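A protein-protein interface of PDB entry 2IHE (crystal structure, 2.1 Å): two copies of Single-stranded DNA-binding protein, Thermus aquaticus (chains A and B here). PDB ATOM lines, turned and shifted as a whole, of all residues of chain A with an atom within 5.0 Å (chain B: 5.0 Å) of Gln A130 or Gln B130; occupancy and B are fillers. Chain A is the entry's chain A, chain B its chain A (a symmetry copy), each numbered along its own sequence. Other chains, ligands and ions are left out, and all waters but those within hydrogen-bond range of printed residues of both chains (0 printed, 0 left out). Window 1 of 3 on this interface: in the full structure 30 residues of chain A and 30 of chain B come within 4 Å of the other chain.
OE1 of Gln A130 lies within hydrogen-bond range of NE2 of Gln B130, at 3.2 Å.
O of Gln A7 sits at hydrogen-bond distance from N of Ile A132. The backbone carbonyl oxygen (O) of Gln A130 is in hydrogen-bond range of the backbone NH (N) of Phe A9. The backbone carbonyl oxygen of Gln B7 sits at hydrogen-bond distance from the backbone NH of Ile B132. The backbone NH (N) of Phe B9 lies within hydrogen-bond range of the backbone carbonyl oxygen (O) of Gln B130 (3.0 Å).
Among the printed residues, merely in contact across the chains: Phe A9 with Ile B132 (3.8 Å) and Ile A132 with Phe B9 (3.8 Å).
Printed residues of chain A within 4 Å of Gln B130: Gln A130 (3.2 Å). Of the printed residues of chain A, Phe B9 touches Ile A132 (3.8 Å). Printed residues of chain B within 4 Å of Ile A132: Phe B9 (3.8 Å). Printed residues of chain A within 4 Å of Ile B132: Phe A9. Of the printed residues of chain B, Phe A9 touches Ile B132 (3.8 Å). Leu B128 touches none of the printed residues of chain A. Val B131 touches none of the printed residues of chain A. The nearest residue of chain B that does not touch Gln A130 is Phe B9 (4.9 Å). The nearest residue of chain A that does not touch Gln B130 is Phe A9 (4.9 Å). The nearest printed residue of chain A that does not touch Phe B9 is Phe A9 (4.6 Å).
Of the 11 printed residues of chain B, 3 touch a printed residue of chain A. Printed residues of chain B that touch a printed residue of chain A: Phe B9, Gln B130 and Ile B132. Hydrophobic or aromatic side chains of chain B that line the printed part of chain A: Phe B9 and Ile B132. Printed residues of chain A that touch a printed residue of chain B: Phe A9, Gln A130 and Ile A132. Hydrophobic or aromatic side chains of chain A that line the printed part of chain B: Phe A9 and Ile A132. Among the printed residues, 3 pairs touch across the chains.
Phe A9 touches Ile B132, and with the chains exchanged Ile A132 touches Phe B9. Gln A130 touches its own counterpart, Gln B130.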
ATOM      1  N   GLN A   7      16.682  18.160  -6.007  1.00  0.00           N
ATOM      2  CA  GLN A   7      15.852  19.279  -6.441  1.00  0.00           C
ATOM      3  C   GLN A   7      16.122  19.774  -7.874  1.00  0.00           C
ATOM      4  O   GLN A   7      17.263  20.035  -8.247  1.00  0.00           O
ATOM      5  CB  GLN A   7      16.035  20.441  -5.464  1.00  0.00           C
ATOM      6  CG  GLN A   7      15.370  20.229  -4.124  1.00  0.00           C
ATOM      7  CD  GLN A   7      14.039  20.939  -4.031  1.00  0.00           C
ATOM      8  OE1 GLN A   7      13.180  20.568  -3.230  1.00  0.00           O
ATOM      9  NE2 GLN A   7      13.864  21.977  -4.843  1.00  0.00           N
ATOM     10  N   VAL A   8      15.066  19.917  -8.671  1.00  0.00           N
ATOM     11  CA  VAL A   8      15.198  20.399 -10.045  1.00  0.00           C
ATOM     12  C   VAL A   8      14.237  21.559 -10.274  1.00  0.00           C
ATOM     13  O   VAL A   8      13.076  21.497  -9.876  1.00  0.00           O
ATOM     14  CB  VAL A   8      14.881  19.280 -11.085  1.00  0.00           C
ATOM     15  CG1 VAL A   8      14.950  19.841 -12.491  1.00  0.00           C
ATOM     16  CG2 VAL A   8      15.867  18.128 -10.948  1.00  0.00           C
ATOM     17  N   PHE A   9      14.737  22.632 -10.881  1.00  0.00           N
ATOM     18  CA  PHE A   9      13.921  23.804 -11.210  1.00  0.00           C
ATOM     19  C   PHE A   9      14.116  24.122 -12.680  1.00  0.00           C
ATOM     20  O   PHE A   9      15.248  24.309 -13.129  1.00  0.00           O
ATOM     21  CB  PHE A   9      14.341  25.018 -10.408  1.00  0.00           C
ATOM     22  CG  PHE A   9      13.975  24.942  -8.976  1.00  0.00           C
ATOM     23  CD1 PHE A   9      14.961  24.888  -8.001  1.00  0.00           C
ATOM     24  CD2 PHE A   9      12.645  24.952  -8.589  1.00  0.00           C
ATOM     25  CE1 PHE A   9      14.631  24.852  -6.649  1.00  0.00           C
ATOM     26  CE2 PHE A   9      12.301  24.918  -7.236  1.00  0.00           C
ATOM     27  CZ  PHE A   9      13.301  24.868  -6.264  1.00  0.00           C
ATOM     28  N   LEU A  10      13.017  24.187 -13.426  1.00  0.00           N
ATOM     29  CA  LEU A  10      13.090  24.499 -14.848  1.00  0.00           C
ATOM     30  C   LEU A  10      12.065  25.534 -15.271  1.00  0.00           C
ATOM     31  O   LEU A  10      11.045  25.713 -14.627  1.00  0.00           O
ATOM     32  CB  LEU A  10      12.835  23.250 -15.697  1.00  0.00           C
ATOM     33  CG  LEU A  10      13.676  21.987 -15.610  1.00  0.00           C
ATOM     34  CD1 LEU A  10      13.019  20.914 -16.470  1.00  0.00           C
ATOM     35  CD2 LEU A  10      15.084  22.263 -16.074  1.00  0.00           C
ATOM     36  N   LEU A 128      15.315  28.508 -17.630  1.00  0.00           N
ATOM     37  CA  LEU A 128      15.947  28.239 -16.351  1.00  0.00           C
ATOM     38  C   LEU A 128      16.184  26.743 -16.270  1.00  0.00           C
ATOM     39  O   LEU A 128      15.297  25.951 -16.557  1.00  0.00           O
ATOM     40  CB  LEU A 128      15.039  28.670 -15.211  1.00  0.00           C
ATOM     41  CG  LEU A 128      15.640  28.416 -13.839  1.00  0.00           C
ATOM     42  CD1 LEU A 128      16.821  29.342 -13.654  1.00  0.00           C
ATOM     43  CD2 LEU A 128      14.612  28.648 -12.759  1.00  0.00           C
ATOM     44  N   ASN A 129      17.391  26.358 -15.886  1.00  0.00           N
ATOM     45  CA  ASN A 129      17.743  24.954 -15.778  1.00  0.00           C
ATOM     46  C   ASN A 129      18.737  24.827 -14.633  1.00  0.00           C
ATOM     47  O   ASN A 129      19.930  25.088 -14.800  1.00  0.00           O
ATOM     48  CB  ASN A 129      18.380  24.478 -17.084  1.00  0.00           C
ATOM     49  CG  ASN A 129      18.730  23.005 -17.066  1.00  0.00           C
ATOM     50  OD1 ASN A 129      18.701  22.349 -16.021  1.00  0.00           O
ATOM     51  ND2 ASN A 129      19.079  22.478 -18.228  1.00  0.00           N
ATOM     52  N   GLN A 130      18.242  24.429 -13.465  1.00  0.00           N
ATOM     53  CA  GLN A 130      19.100  24.293 -12.298  1.00  0.00           C
ATOM     54  C   GLN A 130      18.825  23.000 -11.554  1.00  0.00           C
ATOM     55  O   GLN A 130      17.676  22.615 -11.357  1.00  0.00           O
ATOM     56  CB  GLN A 130      18.876  25.477 -11.367  1.00  0.00           C
ATOM     57  CG  GLN A 130      19.759  25.478 -10.140  1.00  0.00           C
ATOM     58  CD  GLN A 130      19.059  26.106  -8.942  1.00  0.00           C
ATOM     59  OE1 GLN A 130      18.341  27.104  -9.087  1.00  0.00           O
ATOM     60  NE2 GLN A 130      19.267  25.529  -7.749  1.00  0.00           N
ATOM     61  N   VAL A 131      19.890  22.328 -11.145  1.00  0.00           N
ATOM     62  CA  VAL A 131      19.775  21.081 -10.404  1.00  0.00           C
ATOM     63  C   VAL A 131      20.696  21.130  -9.182  1.00  0.00           C
ATOM     64  O   VAL A 131      21.793  21.676  -9.253  1.00  0.00           O
ATOM     65  CB  VAL A 131      20.165  19.870 -11.300  1.00  0.00           C
ATOM     66  CG1 VAL A 131      20.095  18.572 -10.515  1.00  0.00           C
ATOM     67  CG2 VAL A 131      19.234  19.797 -12.491  1.00  0.00           C
ATOM     68  N   ILE A 132      20.224  20.597  -8.053  1.00  0.00           N
ATOM     69  CA  ILE A 132      21.024  20.522  -6.821  1.00  0.00           C
ATOM     70  C   ILE A 132      20.858  19.121  -6.206  1.00  0.00           C
ATOM     71  O   ILE A 132      19.755  18.705  -5.854  1.00  0.00           O
ATOM     72  CB  ILE A 132      20.641  21.638  -5.799  1.00  0.00           C
ATOM     73  CG1 ILE A 132      21.465  21.453  -4.527  1.00  0.00           C
ATOM     74  CG2 ILE A 132      19.156  21.632  -5.512  1.00  0.00           C
ATOM     75  CD1 ILE A 132      21.442  22.637  -3.590  1.00  0.00           C
ATOM     76  N   GLY A 199      24.333  22.208 -10.596  1.00  0.00           N
ATOM     77  CA  GLY A 199      24.534  22.414 -12.018  1.00  0.00           C
ATOM     78  C   GLY A 199      23.267  22.466 -12.859  1.00  0.00           C
ATOM     79  O   GLY A 199      22.216  22.949 -12.442  1.00  0.00           O
ATOM     80  N   ARG A 200      23.369  21.953 -14.070  1.00  0.00           N
ATOM     81  CA  ARG A 200      22.239  21.959 -14.971  1.00  0.00           C
ATOM     82  C   ARG A 200      22.064  20.590 -15.615  1.00  0.00           C
ATOM     83  O   ARG A 200      23.021  19.833 -15.771  1.00  0.00           O
ATOM     84  CB  ARG A 200      22.442  23.057 -16.023  1.00  0.00           C
ATOM     85  CG  ARG A 200      23.860  23.152 -16.568  1.00  0.00           C
ATOM     86  CD  ARG A 200      24.071  24.431 -17.376  1.00  0.00           C
ATOM     87  NE  ARG A 200      25.390  24.502 -18.012  1.00  0.00           N
ATOM     88  CZ  ARG A 200      25.744  23.822 -19.104  1.00  0.00           C
ATOM     89  NH1 ARG A 200      24.881  23.008 -19.703  1.00  0.00           N
ATOM     90  NH2 ARG A 200      26.966  23.960 -19.602  1.00  0.00           N
ATOM     91  N   GLN B   7      12.068  28.735  -0.656  1.00  0.00           N
ATOM     92  CA  GLN B   7      13.328  28.001  -0.611  1.00  0.00           C
ATOM     93  C   GLN B   7      14.593  28.880  -0.569  1.00  0.00           C
ATOM     94  O   GLN B   7      14.758  29.788  -1.380  1.00  0.00           O
ATOM     95  CB  GLN B   7      13.403  27.070  -1.822  1.00  0.00           C
ATOM     96  CG  GLN B   7      12.490  25.869  -1.731  1.00  0.00           C
ATOM     97  CD  GLN B   7      13.226  24.628  -1.286  1.00  0.00           C
ATOM     98  OE1 GLN B   7      12.624  23.690  -0.761  1.00  0.00           O
ATOM     99  NE2 GLN B   7      14.538  24.607  -1.503  1.00  0.00           N
ATOM    100  N   VAL B   8      15.492  28.597   0.370  1.00  0.00           N
ATOM    101  CA  VAL B   8      16.739  29.350   0.493  1.00  0.00           C
ATOM    102  C   VAL B   8      17.918  28.384   0.526  1.00  0.00           C
ATOM    103  O   VAL B   8      17.876  27.369   1.217  1.00  0.00           O
ATOM    104  CB  VAL B   8      16.770  30.212   1.793  1.00  0.00           C
ATOM    105  CG1 VAL B   8      18.108  30.910   1.924  1.00  0.00           C
ATOM    106  CG2 VAL B   8      15.655  31.248   1.773  1.00  0.00           C
ATOM    107  N   PHE B   9      18.951  28.683  -0.257  1.00  0.00           N
ATOM    108  CA  PHE B   9      20.171  27.874  -0.295  1.00  0.00           C
ATOM    109  C   PHE B   9      21.359  28.792  -0.078  1.00  0.00           C
ATOM    110  O   PHE B   9      21.528  29.770  -0.809  1.00  0.00           O
ATOM    111  CB  PHE B   9      20.347  27.192  -1.636  1.00  0.00           C
ATOM    112  CG  PHE B   9      19.391  26.086  -1.871  1.00  0.00           C
ATOM    113  CD1 PHE B   9      18.446  26.176  -2.883  1.00  0.00           C
ATOM    114  CD2 PHE B   9      19.447  24.935  -1.103  1.00  0.00           C
ATOM    115  CE1 PHE B   9      17.566  25.129  -3.138  1.00  0.00           C
ATOM    116  CE2 PHE B   9      18.570  23.875  -1.349  1.00  0.00           C
ATOM    117  CZ  PHE B   9      17.626  23.977  -2.372  1.00  0.00           C
ATOM    118  N   LEU B  10      22.179  28.479   0.920  1.00  0.00           N
ATOM    119  CA  LEU B  10      23.358  29.287   1.208  1.00  0.00           C
ATOM    120  C   LEU B  10      24.600  28.446   1.434  1.00  0.00           C
ATOM    121  O   LEU B  10      24.520  27.282   1.788  1.00  0.00           O
ATOM    122  CB  LEU B  10      23.153  30.124   2.473  1.00  0.00           C
ATOM    123  CG  LEU B  10      22.031  31.135   2.641  1.00  0.00           C
ATOM    124  CD1 LEU B  10      22.049  31.637   4.080  1.00  0.00           C
ATOM    125  CD2 LEU B  10      22.206  32.276   1.671  1.00  0.00           C
ATOM    126  N   LEU B 128      27.488  30.967  -1.772  1.00  0.00           N
ATOM    127  CA  LEU B 128      26.271  30.712  -2.519  1.00  0.00           C
ATOM    128  C   LEU B 128      25.138  31.405  -1.788  1.00  0.00           C
ATOM    129  O   LEU B 128      25.006  31.286  -0.577  1.00  0.00           O
ATOM    130  CB  LEU B 128      25.993  29.219  -2.585  1.00  0.00           C
ATOM    131  CG  LEU B 128      24.728  28.879  -3.355  1.00  0.00           C
ATOM    132  CD1 LEU B 128      24.952  29.211  -4.813  1.00  0.00           C
ATOM    133  CD2 LEU B 128      24.384  27.419  -3.191  1.00  0.00           C
ATOM    134  N   ASN B 129      24.323  32.141  -2.528  1.00  0.00           N
ATOM    135  CA  ASN B 129      23.207  32.861  -1.943  1.00  0.00           C
ATOM    136  C   ASN B 129      22.092  32.881  -2.979  1.00  0.00           C
ATOM    137  O   ASN B 129      22.103  33.697  -3.903  1.00  0.00           O
ATOM    138  CB  ASN B 129      23.633  34.289  -1.601  1.00  0.00           C
ATOM    139  CG  ASN B 129      22.532  35.090  -0.938  1.00  0.00           C
ATOM    140  OD1 ASN B 129      21.369  34.679  -0.902  1.00  0.00           O
ATOM    141  ND2 ASN B 129      22.893  36.253  -0.420  1.00  0.00           N
ATOM    142  N   GLN B 130      21.131  31.975  -2.826  1.00  0.00           N
ATOM    143  CA  GLN B 130      20.027  31.891  -3.771  1.00  0.00           C
ATOM    144  C   GLN B 130      18.696  31.746  -3.059  1.00  0.00           C
ATOM    145  O   GLN B 130      18.571  30.990  -2.100  1.00  0.00           O
ATOM    146  CB  GLN B 130      20.245  30.702  -4.697  1.00  0.00           C
ATOM    147  CG  GLN B 130      19.189  30.545  -5.766  1.00  0.00           C
ATOM    148  CD  GLN B 130      18.955  29.082  -6.118  1.00  0.00           C
ATOM    149  OE1 GLN B 130      19.907  28.293  -6.185  1.00  0.00           O
ATOM    150  NE2 GLN B 130      17.687  28.710  -6.350  1.00  0.00           N
ATOM    151  N   VAL B 131      17.702  32.482  -3.533  1.00  0.00           N
ATOM    152  CA  VAL B 131      16.366  32.430  -2.958  1.00  0.00           C
ATOM    153  C   VAL B 131      15.336  32.283  -4.081  1.00  0.00           C
ATOM    154  O   VAL B 131      15.498  32.864  -5.151  1.00  0.00           O
ATOM    155  CB  VAL B 131      16.067  33.722  -2.143  1.00  0.00           C
ATOM    156  CG1 VAL B 131      14.655  33.693  -1.585  1.00  0.00           C
ATOM    157  CG2 VAL B 131      17.061  33.851  -1.010  1.00  0.00           C
ATOM    158  N   ILE B 132      14.304  31.470  -3.848  1.00  0.00           N
ATOM    159  CA  ILE B 132      13.212  31.283  -4.814  1.00  0.00           C
ATOM    160  C   ILE B 132      11.870  31.335  -4.062  1.00  0.00           C
ATOM    161  O   ILE B 132      11.604  30.526  -3.173  1.00  0.00           O
ATOM    162  CB  ILE B 132      13.358  29.955  -5.621  1.00  0.00           C
ATOM    163  CG1 ILE B 132      12.156  29.803  -6.551  1.00  0.00           C
ATOM    164  CG2 ILE B 132      13.508  28.767  -4.698  1.00  0.00           C
ATOM    165  CD1 ILE B 132      12.322  28.746  -7.618  1.00  0.00           C
ATOM    166  N   GLY B 199      16.186  35.221  -6.734  1.00  0.00           N
ATOM    167  CA  GLY B 199      17.262  36.158  -6.470  1.00  0.00           C
ATOM    168  C   GLY B 199      18.179  35.794  -5.312  1.00  0.00           C
ATOM    169  O   GLY B 199      18.470  34.630  -5.040  1.00  0.00           O
ATOM    170  N   ARG B 200      18.642  36.812  -4.612  1.00  0.00           N
ATOM    171  CA  ARG B 200      19.538  36.596  -3.499  1.00  0.00           C
ATOM    172  C   ARG B 200      19.090  37.407  -2.290  1.00  0.00           C
ATOM    173  O   ARG B 200      18.453  38.452  -2.425  1.00  0.00           O
ATOM    174  CB  ARG B 200      20.965  36.958  -3.925  1.00  0.00           C
ATOM    175  CG  ARG B 200      21.070  38.226  -4.761  1.00  0.00           C
ATOM    176  CD  ARG B 200      22.452  38.372  -5.396  1.00  0.00           C
ATOM    177  NE  ARG B 200      22.627  39.639  -6.114  1.00  0.00           N
ATOM    178  CZ  ARG B 200      22.833  40.820  -5.531  1.00  0.00           C
ATOM    179  NH1 ARG B 200      22.896  40.918  -4.207  1.00  0.00           N
ATOM    180  NH2 ARG B 200      22.981  41.909  -6.274  1.00  0.00           N
